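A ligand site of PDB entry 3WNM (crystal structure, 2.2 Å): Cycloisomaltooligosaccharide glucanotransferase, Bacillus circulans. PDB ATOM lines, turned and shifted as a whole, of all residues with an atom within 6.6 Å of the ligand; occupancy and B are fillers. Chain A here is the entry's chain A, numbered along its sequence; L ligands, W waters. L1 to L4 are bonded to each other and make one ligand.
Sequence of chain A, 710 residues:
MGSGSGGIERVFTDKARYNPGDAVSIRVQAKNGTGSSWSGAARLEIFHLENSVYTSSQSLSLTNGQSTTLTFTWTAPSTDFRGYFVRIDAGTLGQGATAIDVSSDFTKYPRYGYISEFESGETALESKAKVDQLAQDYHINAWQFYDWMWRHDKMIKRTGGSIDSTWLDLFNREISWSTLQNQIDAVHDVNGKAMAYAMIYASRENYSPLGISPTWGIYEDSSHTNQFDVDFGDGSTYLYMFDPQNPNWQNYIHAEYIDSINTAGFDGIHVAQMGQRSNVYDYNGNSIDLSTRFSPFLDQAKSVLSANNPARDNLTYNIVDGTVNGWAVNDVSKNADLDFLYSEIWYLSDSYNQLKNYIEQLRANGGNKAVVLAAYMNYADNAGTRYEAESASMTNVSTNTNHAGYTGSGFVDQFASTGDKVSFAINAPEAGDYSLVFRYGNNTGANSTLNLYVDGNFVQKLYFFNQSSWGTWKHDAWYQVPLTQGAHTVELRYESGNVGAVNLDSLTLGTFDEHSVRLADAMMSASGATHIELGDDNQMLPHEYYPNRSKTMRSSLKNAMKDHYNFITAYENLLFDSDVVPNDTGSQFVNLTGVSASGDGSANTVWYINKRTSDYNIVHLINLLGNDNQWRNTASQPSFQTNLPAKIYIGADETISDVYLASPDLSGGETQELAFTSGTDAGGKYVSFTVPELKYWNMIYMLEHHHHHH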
ATOM      1  N   ASN A 400       6.976  30.220 -25.828  1.00  0.00           N
ATOM      2  CA  ASN A 400       8.085  30.307 -24.920  1.00  0.00           C
ATOM      3  C   ASN A 400       9.312  29.599 -25.479  1.00  0.00           C
ATOM      4  O   ASN A 400       9.255  28.995 -26.552  1.00  0.00           O
ATOM      5  CB  ASN A 400       7.710  29.746 -23.546  1.00  0.00           C
ATOM      6  CG  ASN A 400       8.391  30.497 -22.428  1.00  0.00           C
ATOM      7  OD1 ASN A 400       9.527  30.987 -22.595  1.00  0.00           O
ATOM      8  ND2 ASN A 400       7.723  30.619 -21.293  1.00  0.00           N
ATOM      9  N   ASN A 402      11.778  28.431 -22.825  1.00  0.00           N
ATOM     10  CA  ASN A 402      12.457  28.249 -21.531  1.00  0.00           C
ATOM     11  C   ASN A 402      12.624  26.792 -21.071  1.00  0.00           C
ATOM     12  O   ASN A 402      12.704  26.523 -19.881  1.00  0.00           O
ATOM     13  CB  ASN A 402      11.735  29.067 -20.461  1.00  0.00           C
ATOM     14  CG  ASN A 402      10.354  28.536 -20.161  1.00  0.00           C
ATOM     15  OD1 ASN A 402       9.716  27.931 -21.023  1.00  0.00           O
ATOM     16  ND2 ASN A 402       9.892  28.729 -18.947  1.00  0.00           N
ATOM     17  N   HIS A 403      12.674  25.857 -22.022  1.00  0.00           N
ATOM     18  CA  HIS A 403      13.091  24.469 -21.790  1.00  0.00           C
ATOM     19  C   HIS A 403      13.746  24.026 -23.092  1.00  0.00           C
ATOM     20  O   HIS A 403      13.144  24.139 -24.160  1.00  0.00           O
ATOM     21  CB  HIS A 403      11.919  23.539 -21.518  1.00  0.00           C
ATOM     22  CG  HIS A 403      11.106  23.896 -20.318  1.00  0.00           C
ATOM     23  ND1 HIS A 403      11.605  23.823 -19.041  1.00  0.00           N
ATOM     24  CD2 HIS A 403       9.809  24.277 -20.200  1.00  0.00           C
ATOM     25  CE1 HIS A 403      10.659  24.169 -18.178  1.00  0.00           C
ATOM     26  NE2 HIS A 403       9.560  24.457 -18.854  1.00  0.00           N
ATOM     27  N   PHE A 411       8.210  27.033 -28.487  1.00  0.00           N
ATOM     28  CA  PHE A 411       7.076  26.151 -28.353  1.00  0.00           C
ATOM     29  C   PHE A 411       5.903  26.873 -27.684  1.00  0.00           C
ATOM     30  O   PHE A 411       6.052  28.001 -27.232  1.00  0.00           O
ATOM     31  CB  PHE A 411       7.447  24.938 -27.507  1.00  0.00           C
ATOM     32  CG  PHE A 411       8.002  25.291 -26.156  1.00  0.00           C
ATOM     33  CD1 PHE A 411       9.367  25.512 -25.990  1.00  0.00           C
ATOM     34  CD2 PHE A 411       7.166  25.382 -25.050  1.00  0.00           C
ATOM     35  CE1 PHE A 411       9.881  25.831 -24.732  1.00  0.00           C
ATOM     36  CE2 PHE A 411       7.675  25.693 -23.796  1.00  0.00           C
ATOM     37  CZ  PHE A 411       9.035  25.921 -23.635  1.00  0.00           C
ATOM     38  N   VAL A 412       4.761  26.198 -27.602  1.00  0.00           N
ATOM     39  CA  VAL A 412       3.608  26.740 -26.930  1.00  0.00           C
ATOM     40  C   VAL A 412       3.503  26.121 -25.542  1.00  0.00           C
ATOM     41  O   VAL A 412       3.513  24.899 -25.412  1.00  0.00           O
ATOM     42  CB  VAL A 412       2.317  26.491 -27.759  1.00  0.00           C
ATOM     43  CG1 VAL A 412       1.065  26.857 -26.974  1.00  0.00           C
ATOM     44  CG2 VAL A 412       2.389  27.290 -29.069  1.00  0.00           C
ATOM     45  N   ASP A 413       3.401  26.956 -24.520  1.00  0.00           N
ATOM     46  CA  ASP A 413       3.366  26.470 -23.128  1.00  0.00           C
ATOM     47  C   ASP A 413       2.011  26.658 -22.458  1.00  0.00           C
ATOM     48  O   ASP A 413       1.097  27.253 -23.030  1.00  0.00           O
ATOM     49  CB  ASP A 413       4.456  27.134 -22.294  1.00  0.00           C
ATOM     50  CG  ASP A 413       4.262  28.658 -22.141  1.00  0.00           C
ATOM     51  OD1 ASP A 413       3.201  29.210 -22.510  1.00  0.00           O
ATOM     52  OD2 ASP A 413       5.201  29.298 -21.643  1.00  0.00           O
ATOM     53  N   GLN A 414       1.900  26.120 -21.237  1.00  0.00           N
ATOM     54  CA  GLN A 414       0.746  26.339 -20.390  1.00  0.00           C
ATOM     55  C   GLN A 414      -0.536  26.007 -21.113  1.00  0.00           C
ATOM     56  O   GLN A 414      -1.532  26.720 -20.997  1.00  0.00           O
ATOM     57  CB  GLN A 414       0.701  27.805 -19.924  1.00  0.00           C
ATOM     58  CG  GLN A 414       1.875  28.225 -19.059  1.00  0.00           C
ATOM     59  CD  GLN A 414       1.700  27.859 -17.598  1.00  0.00           C
ATOM     60  OE1 GLN A 414       0.680  27.302 -17.186  1.00  0.00           O
ATOM     61  NE2 GLN A 414       2.696  28.203 -16.788  1.00  0.00           N
ATOM     62  N   PHE A 415      -0.524  24.944 -21.895  1.00  0.00           N
ATOM     63  CA  PHE A 415      -1.713  24.529 -22.600  1.00  0.00           C
ATOM     64  C   PHE A 415      -2.471  23.661 -21.579  1.00  0.00           C
ATOM     65  O   PHE A 415      -2.319  22.428 -21.552  1.00  0.00           O
ATOM     66  CB  PHE A 415      -1.281  23.765 -23.848  1.00  0.00           C
ATOM     67  CG  PHE A 415      -2.339  23.608 -24.899  1.00  0.00           C
ATOM     68  CD1 PHE A 415      -3.670  23.890 -24.654  1.00  0.00           C
ATOM     69  CD2 PHE A 415      -1.981  23.107 -26.147  1.00  0.00           C
ATOM     70  CE1 PHE A 415      -4.625  23.716 -25.639  1.00  0.00           C
ATOM     71  CE2 PHE A 415      -2.931  22.926 -27.127  1.00  0.00           C
ATOM     72  CZ  PHE A 415      -4.249  23.237 -26.877  1.00  0.00           C
ATOM     73  N   ALA A 416      -3.262  24.324 -20.732  1.00  0.00           N
ATOM     74  CA  ALA A 416      -3.720  23.734 -19.476  1.00  0.00           C
ATOM     75  C   ALA A 416      -5.161  24.036 -19.023  1.00  0.00           C
ATOM     76  O   ALA A 416      -5.550  23.593 -17.941  1.00  0.00           O
ATOM     77  CB  ALA A 416      -2.769  24.157 -18.376  1.00  0.00           C
ATOM     78  N   SER A 417      -5.975  24.765 -19.793  1.00  0.00           N
ATOM     79  CA  SER A 417      -7.369  25.039 -19.361  1.00  0.00           C
ATOM     80  C   SER A 417      -8.392  25.227 -20.484  1.00  0.00           C
ATOM     81  O   SER A 417      -8.023  25.519 -21.617  1.00  0.00           O
ATOM     82  CB  SER A 417      -7.466  26.232 -18.387  1.00  0.00           C
ATOM     83  OG  SER A 417      -6.276  27.009 -18.358  1.00  0.00           O
ATOM     84  N   ASN A 443       5.089  17.178 -17.895  1.00  0.00           N
ATOM     85  CA  ASN A 443       5.653  16.788 -16.601  1.00  0.00           C
ATOM     86  C   ASN A 443       4.676  17.174 -15.506  1.00  0.00           C
ATOM     87  O   ASN A 443       5.061  17.666 -14.462  1.00  0.00           O
ATOM     88  CB  ASN A 443       7.029  17.427 -16.384  1.00  0.00           C
ATOM     89  CG  ASN A 443       7.812  16.841 -15.192  1.00  0.00           C
ATOM     90  OD1 ASN A 443       8.585  17.546 -14.544  1.00  0.00           O
ATOM     91  ND2 ASN A 443       7.627  15.557 -14.910  1.00  0.00           N
ATOM     92  N   THR A 444       3.392  16.935 -15.746  1.00  0.00           N
ATOM     93  CA  THR A 444       2.390  17.235 -14.747  1.00  0.00           C
ATOM     94  C   THR A 444       2.315  16.149 -13.696  1.00  0.00           C
ATOM     95  O   THR A 444       1.762  16.373 -12.632  1.00  0.00           O
ATOM     96  CB  THR A 444       1.000  17.350 -15.367  1.00  0.00           C
ATOM     97  OG1 THR A 444       0.696  16.139 -16.079  1.00  0.00           O
ATOM     98  CG2 THR A 444       0.950  18.568 -16.313  1.00  0.00           C
ATOM     99  N   GLY A 445       2.853  14.966 -14.005  1.00  0.00           N
ATOM    100  CA  GLY A 445       2.801  13.815 -13.120  1.00  0.00           C
ATOM    101  C   GLY A 445       1.706  12.841 -13.478  1.00  0.00           C
ATOM    102  O   GLY A 445       1.534  11.829 -12.805  1.00  0.00           O
ATOM    103  N   ALA A 446       0.941  13.150 -14.514  1.00  0.00           N
ATOM    104  CA  ALA A 446       0.003  12.193 -15.061  1.00  0.00           C
ATOM    105  C   ALA A 446      -0.192  12.474 -16.524  1.00  0.00           C
ATOM    106  O   ALA A 446       0.280  13.487 -17.037  1.00  0.00           O
ATOM    107  CB  ALA A 446      -1.322  12.275 -14.329  1.00  0.00           C
ATOM    108  N   SER A 448      -1.914  13.807 -19.766  1.00  0.00           N
ATOM    109  CA  SER A 448      -2.729  14.978 -20.075  1.00  0.00           C
ATOM    110  C   SER A 448      -3.486  14.644 -21.350  1.00  0.00           C
ATOM    111  O   SER A 448      -3.085  13.708 -22.081  1.00  0.00           O
ATOM    112  CB  SER A 448      -1.855  16.212 -20.228  1.00  0.00           C
ATOM    113  OG  SER A 448      -0.977  16.338 -19.124  1.00  0.00           O
ATOM    114  N   TRP A 470      10.426  18.677 -17.908  1.00  0.00           N
ATOM    115  CA  TRP A 470       9.766  19.483 -18.937  1.00  0.00           C
ATOM    116  C   TRP A 470      10.682  19.672 -20.142  1.00  0.00           C
ATOM    117  O   TRP A 470      10.226  20.095 -21.193  1.00  0.00           O
ATOM    118  CB  TRP A 470       9.321  20.851 -18.390  1.00  0.00           C
ATOM    119  CG  TRP A 470       8.071  20.813 -17.528  1.00  0.00           C
ATOM    120  CD1 TRP A 470       8.015  21.016 -16.184  1.00  0.00           C
ATOM    121  CD2 TRP A 470       6.706  20.614 -17.951  1.00  0.00           C
ATOM    122  NE1 TRP A 470       6.714  20.941 -15.743  1.00  0.00           N
ATOM    123  CE2 TRP A 470       5.895  20.690 -16.795  1.00  0.00           C
ATOM    124  CE3 TRP A 470       6.101  20.361 -19.194  1.00  0.00           C
ATOM    125  CZ2 TRP A 470       4.515  20.519 -16.839  1.00  0.00           C
ATOM    126  CZ3 TRP A 470       4.716  20.205 -19.232  1.00  0.00           C
ATOM    127  CH2 TRP A 470       3.938  20.289 -18.062  1.00  0.00           C
ATOM    128  N   VAL A 499      -7.780  16.871 -19.191  1.00  0.00           N
ATOM    129  CA  VAL A 499      -7.012  16.989 -17.966  1.00  0.00           C
ATOM    130  C   VAL A 499      -5.544  17.317 -18.241  1.00  0.00           C
ATOM    131  O   VAL A 499      -5.014  17.077 -19.322  1.00  0.00           O
ATOM    132  CB  VAL A 499      -7.063  15.689 -17.114  1.00  0.00           C
ATOM    133  CG1 VAL A 499      -8.467  15.463 -16.581  1.00  0.00           C
ATOM    134  CG2 VAL A 499      -6.600  14.474 -17.905  1.00  0.00           C
ATOM    135  N   GLY A 500      -4.905  17.862 -17.220  1.00  0.00           N
ATOM    136  CA  GLY A 500      -3.480  18.103 -17.260  1.00  0.00           C
ATOM    137  C   GLY A 500      -3.085  19.328 -18.042  1.00  0.00           C
ATOM    138  O   GLY A 500      -3.800  20.330 -18.070  1.00  0.00           O
ATOM    139  N   ALA A 501      -1.916  19.233 -18.652  1.00  0.00           N
ATOM    140  CA  ALA A 501      -1.313  20.318 -19.374  1.00  0.00           C
ATOM    141  C   ALA A 501      -0.242  19.723 -20.263  1.00  0.00           C
ATOM    142  O   ALA A 501       0.243  18.626 -19.985  1.00  0.00           O
ATOM    143  CB  ALA A 501      -0.721  21.336 -18.415  1.00  0.00           C
ATOM    144  N   VAL A 502       0.084  20.430 -21.338  1.00  0.00           N
ATOM    145  CA  VAL A 502       1.215  20.059 -22.198  1.00  0.00           C
ATOM    146  C   VAL A 502       1.916  21.313 -22.688  1.00  0.00           C
ATOM    147  O   VAL A 502       1.337  22.421 -22.677  1.00  0.00           O
ATOM    148  CB  VAL A 502       0.806  19.213 -23.437  1.00  0.00           C
ATOM    149  CG1 VAL A 502      -0.091  18.050 -23.041  1.00  0.00           C
ATOM    150  CG2 VAL A 502       0.099  20.068 -24.490  1.00  0.00           C
ATOM    151  N   ASN A 503       3.166  21.157 -23.069  1.00  0.00           N
ATOM    152  CA  ASN A 503       3.841  22.097 -23.951  1.00  0.00           C
ATOM    153  C   ASN A 503       3.782  21.476 -25.342  1.00  0.00           C
ATOM    154  O   ASN A 503       3.857  20.248 -25.489  1.00  0.00           O
ATOM    155  CB  ASN A 503       5.274  22.333 -23.491  1.00  0.00           C
ATOM    156  CG  ASN A 503       5.343  23.133 -22.184  1.00  0.00           C
ATOM    157  OD1 ASN A 503       4.327  23.651 -21.697  1.00  0.00           O
ATOM    158  ND2 ASN A 503       6.528  23.231 -21.612  1.00  0.00           N
HETATM  159  C1  LIG L   1       5.773  29.705 -14.119  1.00  0.00           C
HETATM  160  C2  LIG L   1       4.262  29.837 -14.154  1.00  0.00           C
HETATM  161  C3  LIG L   1       3.551  28.900 -13.183  1.00  0.00           C
HETATM  162  C4  LIG L   1       4.142  27.483 -13.103  1.00  0.00           C
HETATM  163  C5  LIG L   1       5.648  27.401 -13.377  1.00  0.00           C
HETATM  164  C6  LIG L   1       5.981  25.986 -13.862  1.00  0.00           C
HETATM  165  O1  LIG L   1       6.297  30.167 -12.898  1.00  0.00           O
HETATM  166  O2  LIG L   1       3.899  31.167 -13.848  1.00  0.00           O
HETATM  167  O3  LIG L   1       2.206  28.788 -13.595  1.00  0.00           O
HETATM  168  O4  LIG L   1       3.900  26.978 -11.816  1.00  0.00           O
HETATM  169  O5  LIG L   1       6.125  28.350 -14.322  1.00  0.00           O
HETATM  170  O6  LIG L   1       5.512  25.755 -15.181  1.00  0.00           O
HETATM  171  C1  LG2 L   2       5.729  24.403 -15.632  1.00  0.00           C
HETATM  172  C2  LG2 L   2       6.608  24.343 -16.881  1.00  0.00           C
HETATM  173  C3  LG2 L   2       5.878  24.936 -18.095  1.00  0.00           C
HETATM  174  C4  LG2 L   2       4.571  24.204 -18.286  1.00  0.00           C
HETATM  175  C5  LG2 L   2       3.774  24.354 -16.988  1.00  0.00           C
HETATM  176  C6  LG2 L   2       2.402  23.697 -17.052  1.00  0.00           C
HETATM  177  O1  LG2 L   2       7.874  24.956 -16.685  1.00  0.00           O
HETATM  178  O2  LG2 L   2       6.651  24.859 -19.270  1.00  0.00           O
HETATM  179  O3  LG2 L   2       3.882  24.764 -19.379  1.00  0.00           O
HETATM  180  O4  LG2 L   2       4.499  23.774 -15.914  1.00  0.00           O
HETATM  181  O5  LG2 L   2       1.616  24.338 -16.077  1.00  0.00           O
HETATM  182  C1  LG3 L   3       0.411  23.587 -15.779  1.00  0.00           C
HETATM  183  C2  LG3 L   3      -0.562  24.496 -15.035  1.00  0.00           C
HETATM  184  C3  LG3 L   3       0.004  24.887 -13.669  1.00  0.00           C
HETATM  185  C4  LG3 L   3       0.434  23.651 -12.901  1.00  0.00           C
HETATM  186  C5  LG3 L   3       1.257  22.682 -13.760  1.00  0.00           C
HETATM  187  C6  LG3 L   3       1.409  21.353 -13.049  1.00  0.00           C
HETATM  188  O1  LG3 L   3      -0.794  25.659 -15.778  1.00  0.00           O
HETATM  189  O2  LG3 L   3      -0.974  25.581 -12.922  1.00  0.00           O
HETATM  190  O3  LG3 L   3       1.189  24.084 -11.810  1.00  0.00           O
HETATM  191  O4  LG3 L   3       0.624  22.429 -15.013  1.00  0.00           O
HETATM  192  O5  LG3 L   3       0.102  20.810 -12.882  1.00  0.00           O
HETATM  193  C1  LG4 L   4       0.178  19.614 -12.091  1.00  0.00           C
HETATM  194  C2  LG4 L   4      -1.154  18.873 -12.130  1.00  0.00           C
HETATM  195  C3  LG4 L   4      -2.204  19.705 -11.407  1.00  0.00           C
HETATM  196  C4  LG4 L   4      -1.803  19.946  -9.963  1.00  0.00           C
HETATM  197  C5  LG4 L   4      -0.338  20.337  -9.775  1.00  0.00           C
HETATM  198  C6  LG4 L   4       0.090  19.826  -8.396  1.00  0.00           C
HETATM  199  O1  LG4 L   4      -1.551  18.587 -13.454  1.00  0.00           O
HETATM  200  O2  LG4 L   4      -3.433  19.005 -11.419  1.00  0.00           O
HETATM  201  O3  LG4 L   4      -2.599  20.980  -9.441  1.00  0.00           O
HETATM  202  O4  LG4 L   4       0.581  19.841 -10.735  1.00  0.00           O
HETATM  203  O5  LG4 L   4       1.328  20.388  -8.040  1.00  0.00           O
HETATM  204  O   HOH W   1      -3.179  16.480 -13.791  1.00  0.00           O
HETATM  205  O   HOH W   2      -1.970  20.982 -15.024  1.00  0.00           O
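Residues that only touch the ligand: Trp 470 (3.4 Å), Thr 444 (3.4 Å), Ala 416 (3.6 Å), Ala 501 (3.6 Å) and Asp 413 (3.8 Å). Hydrophobic or aromatic side chains within 4 Å of the ligand: His 403, Ala 416, Trp 470 and Ala 501. Of the 21 residues printed, 8 come within 4 Å of the ligand. Along chain A the residues within 4 Å of the ligand span positions 403 to 503. The nearest printed residue that does not touch the ligand is Gly 500 (4.3 Å).
The side-chain amide oxygen (OD1) of Asn 503 lies within hydrogen-bond range of an oxygen (O3) of LG2 L2 (2.6 Å). The backbone NH (N) of Gln 414 is in hydrogen-bond range of an oxygen (O3) of LG2 L2, 3.0 Å away. OE1 of Gln 414 sits at hydrogen-bond distance from O1 of LG3 L3, 2.6 Å away. O1 of LG2 L2 is in hydrogen-bond range of NE2 of His 403.
OD1 of Asn 503 sits at hydrogen-bond distance from N of Gln 414 (3.5 Å). The side-chain hydroxyl of Thr 444 lies within hydrogen-bond range of the backbone carbonyl oxygen of Ala 446, 2.9 Å away. OG of Ser 448 sits at hydrogen-bond distance from OG1 of Thr 444, at 3.5 Å. O of Ala 501 sits at hydrogen-bond distance from OG of Ser 448 (2.7 Å). OD2 of Asp 413 lies within hydrogen-bond range of ND2 of Asn 400, at 2.9 Å.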
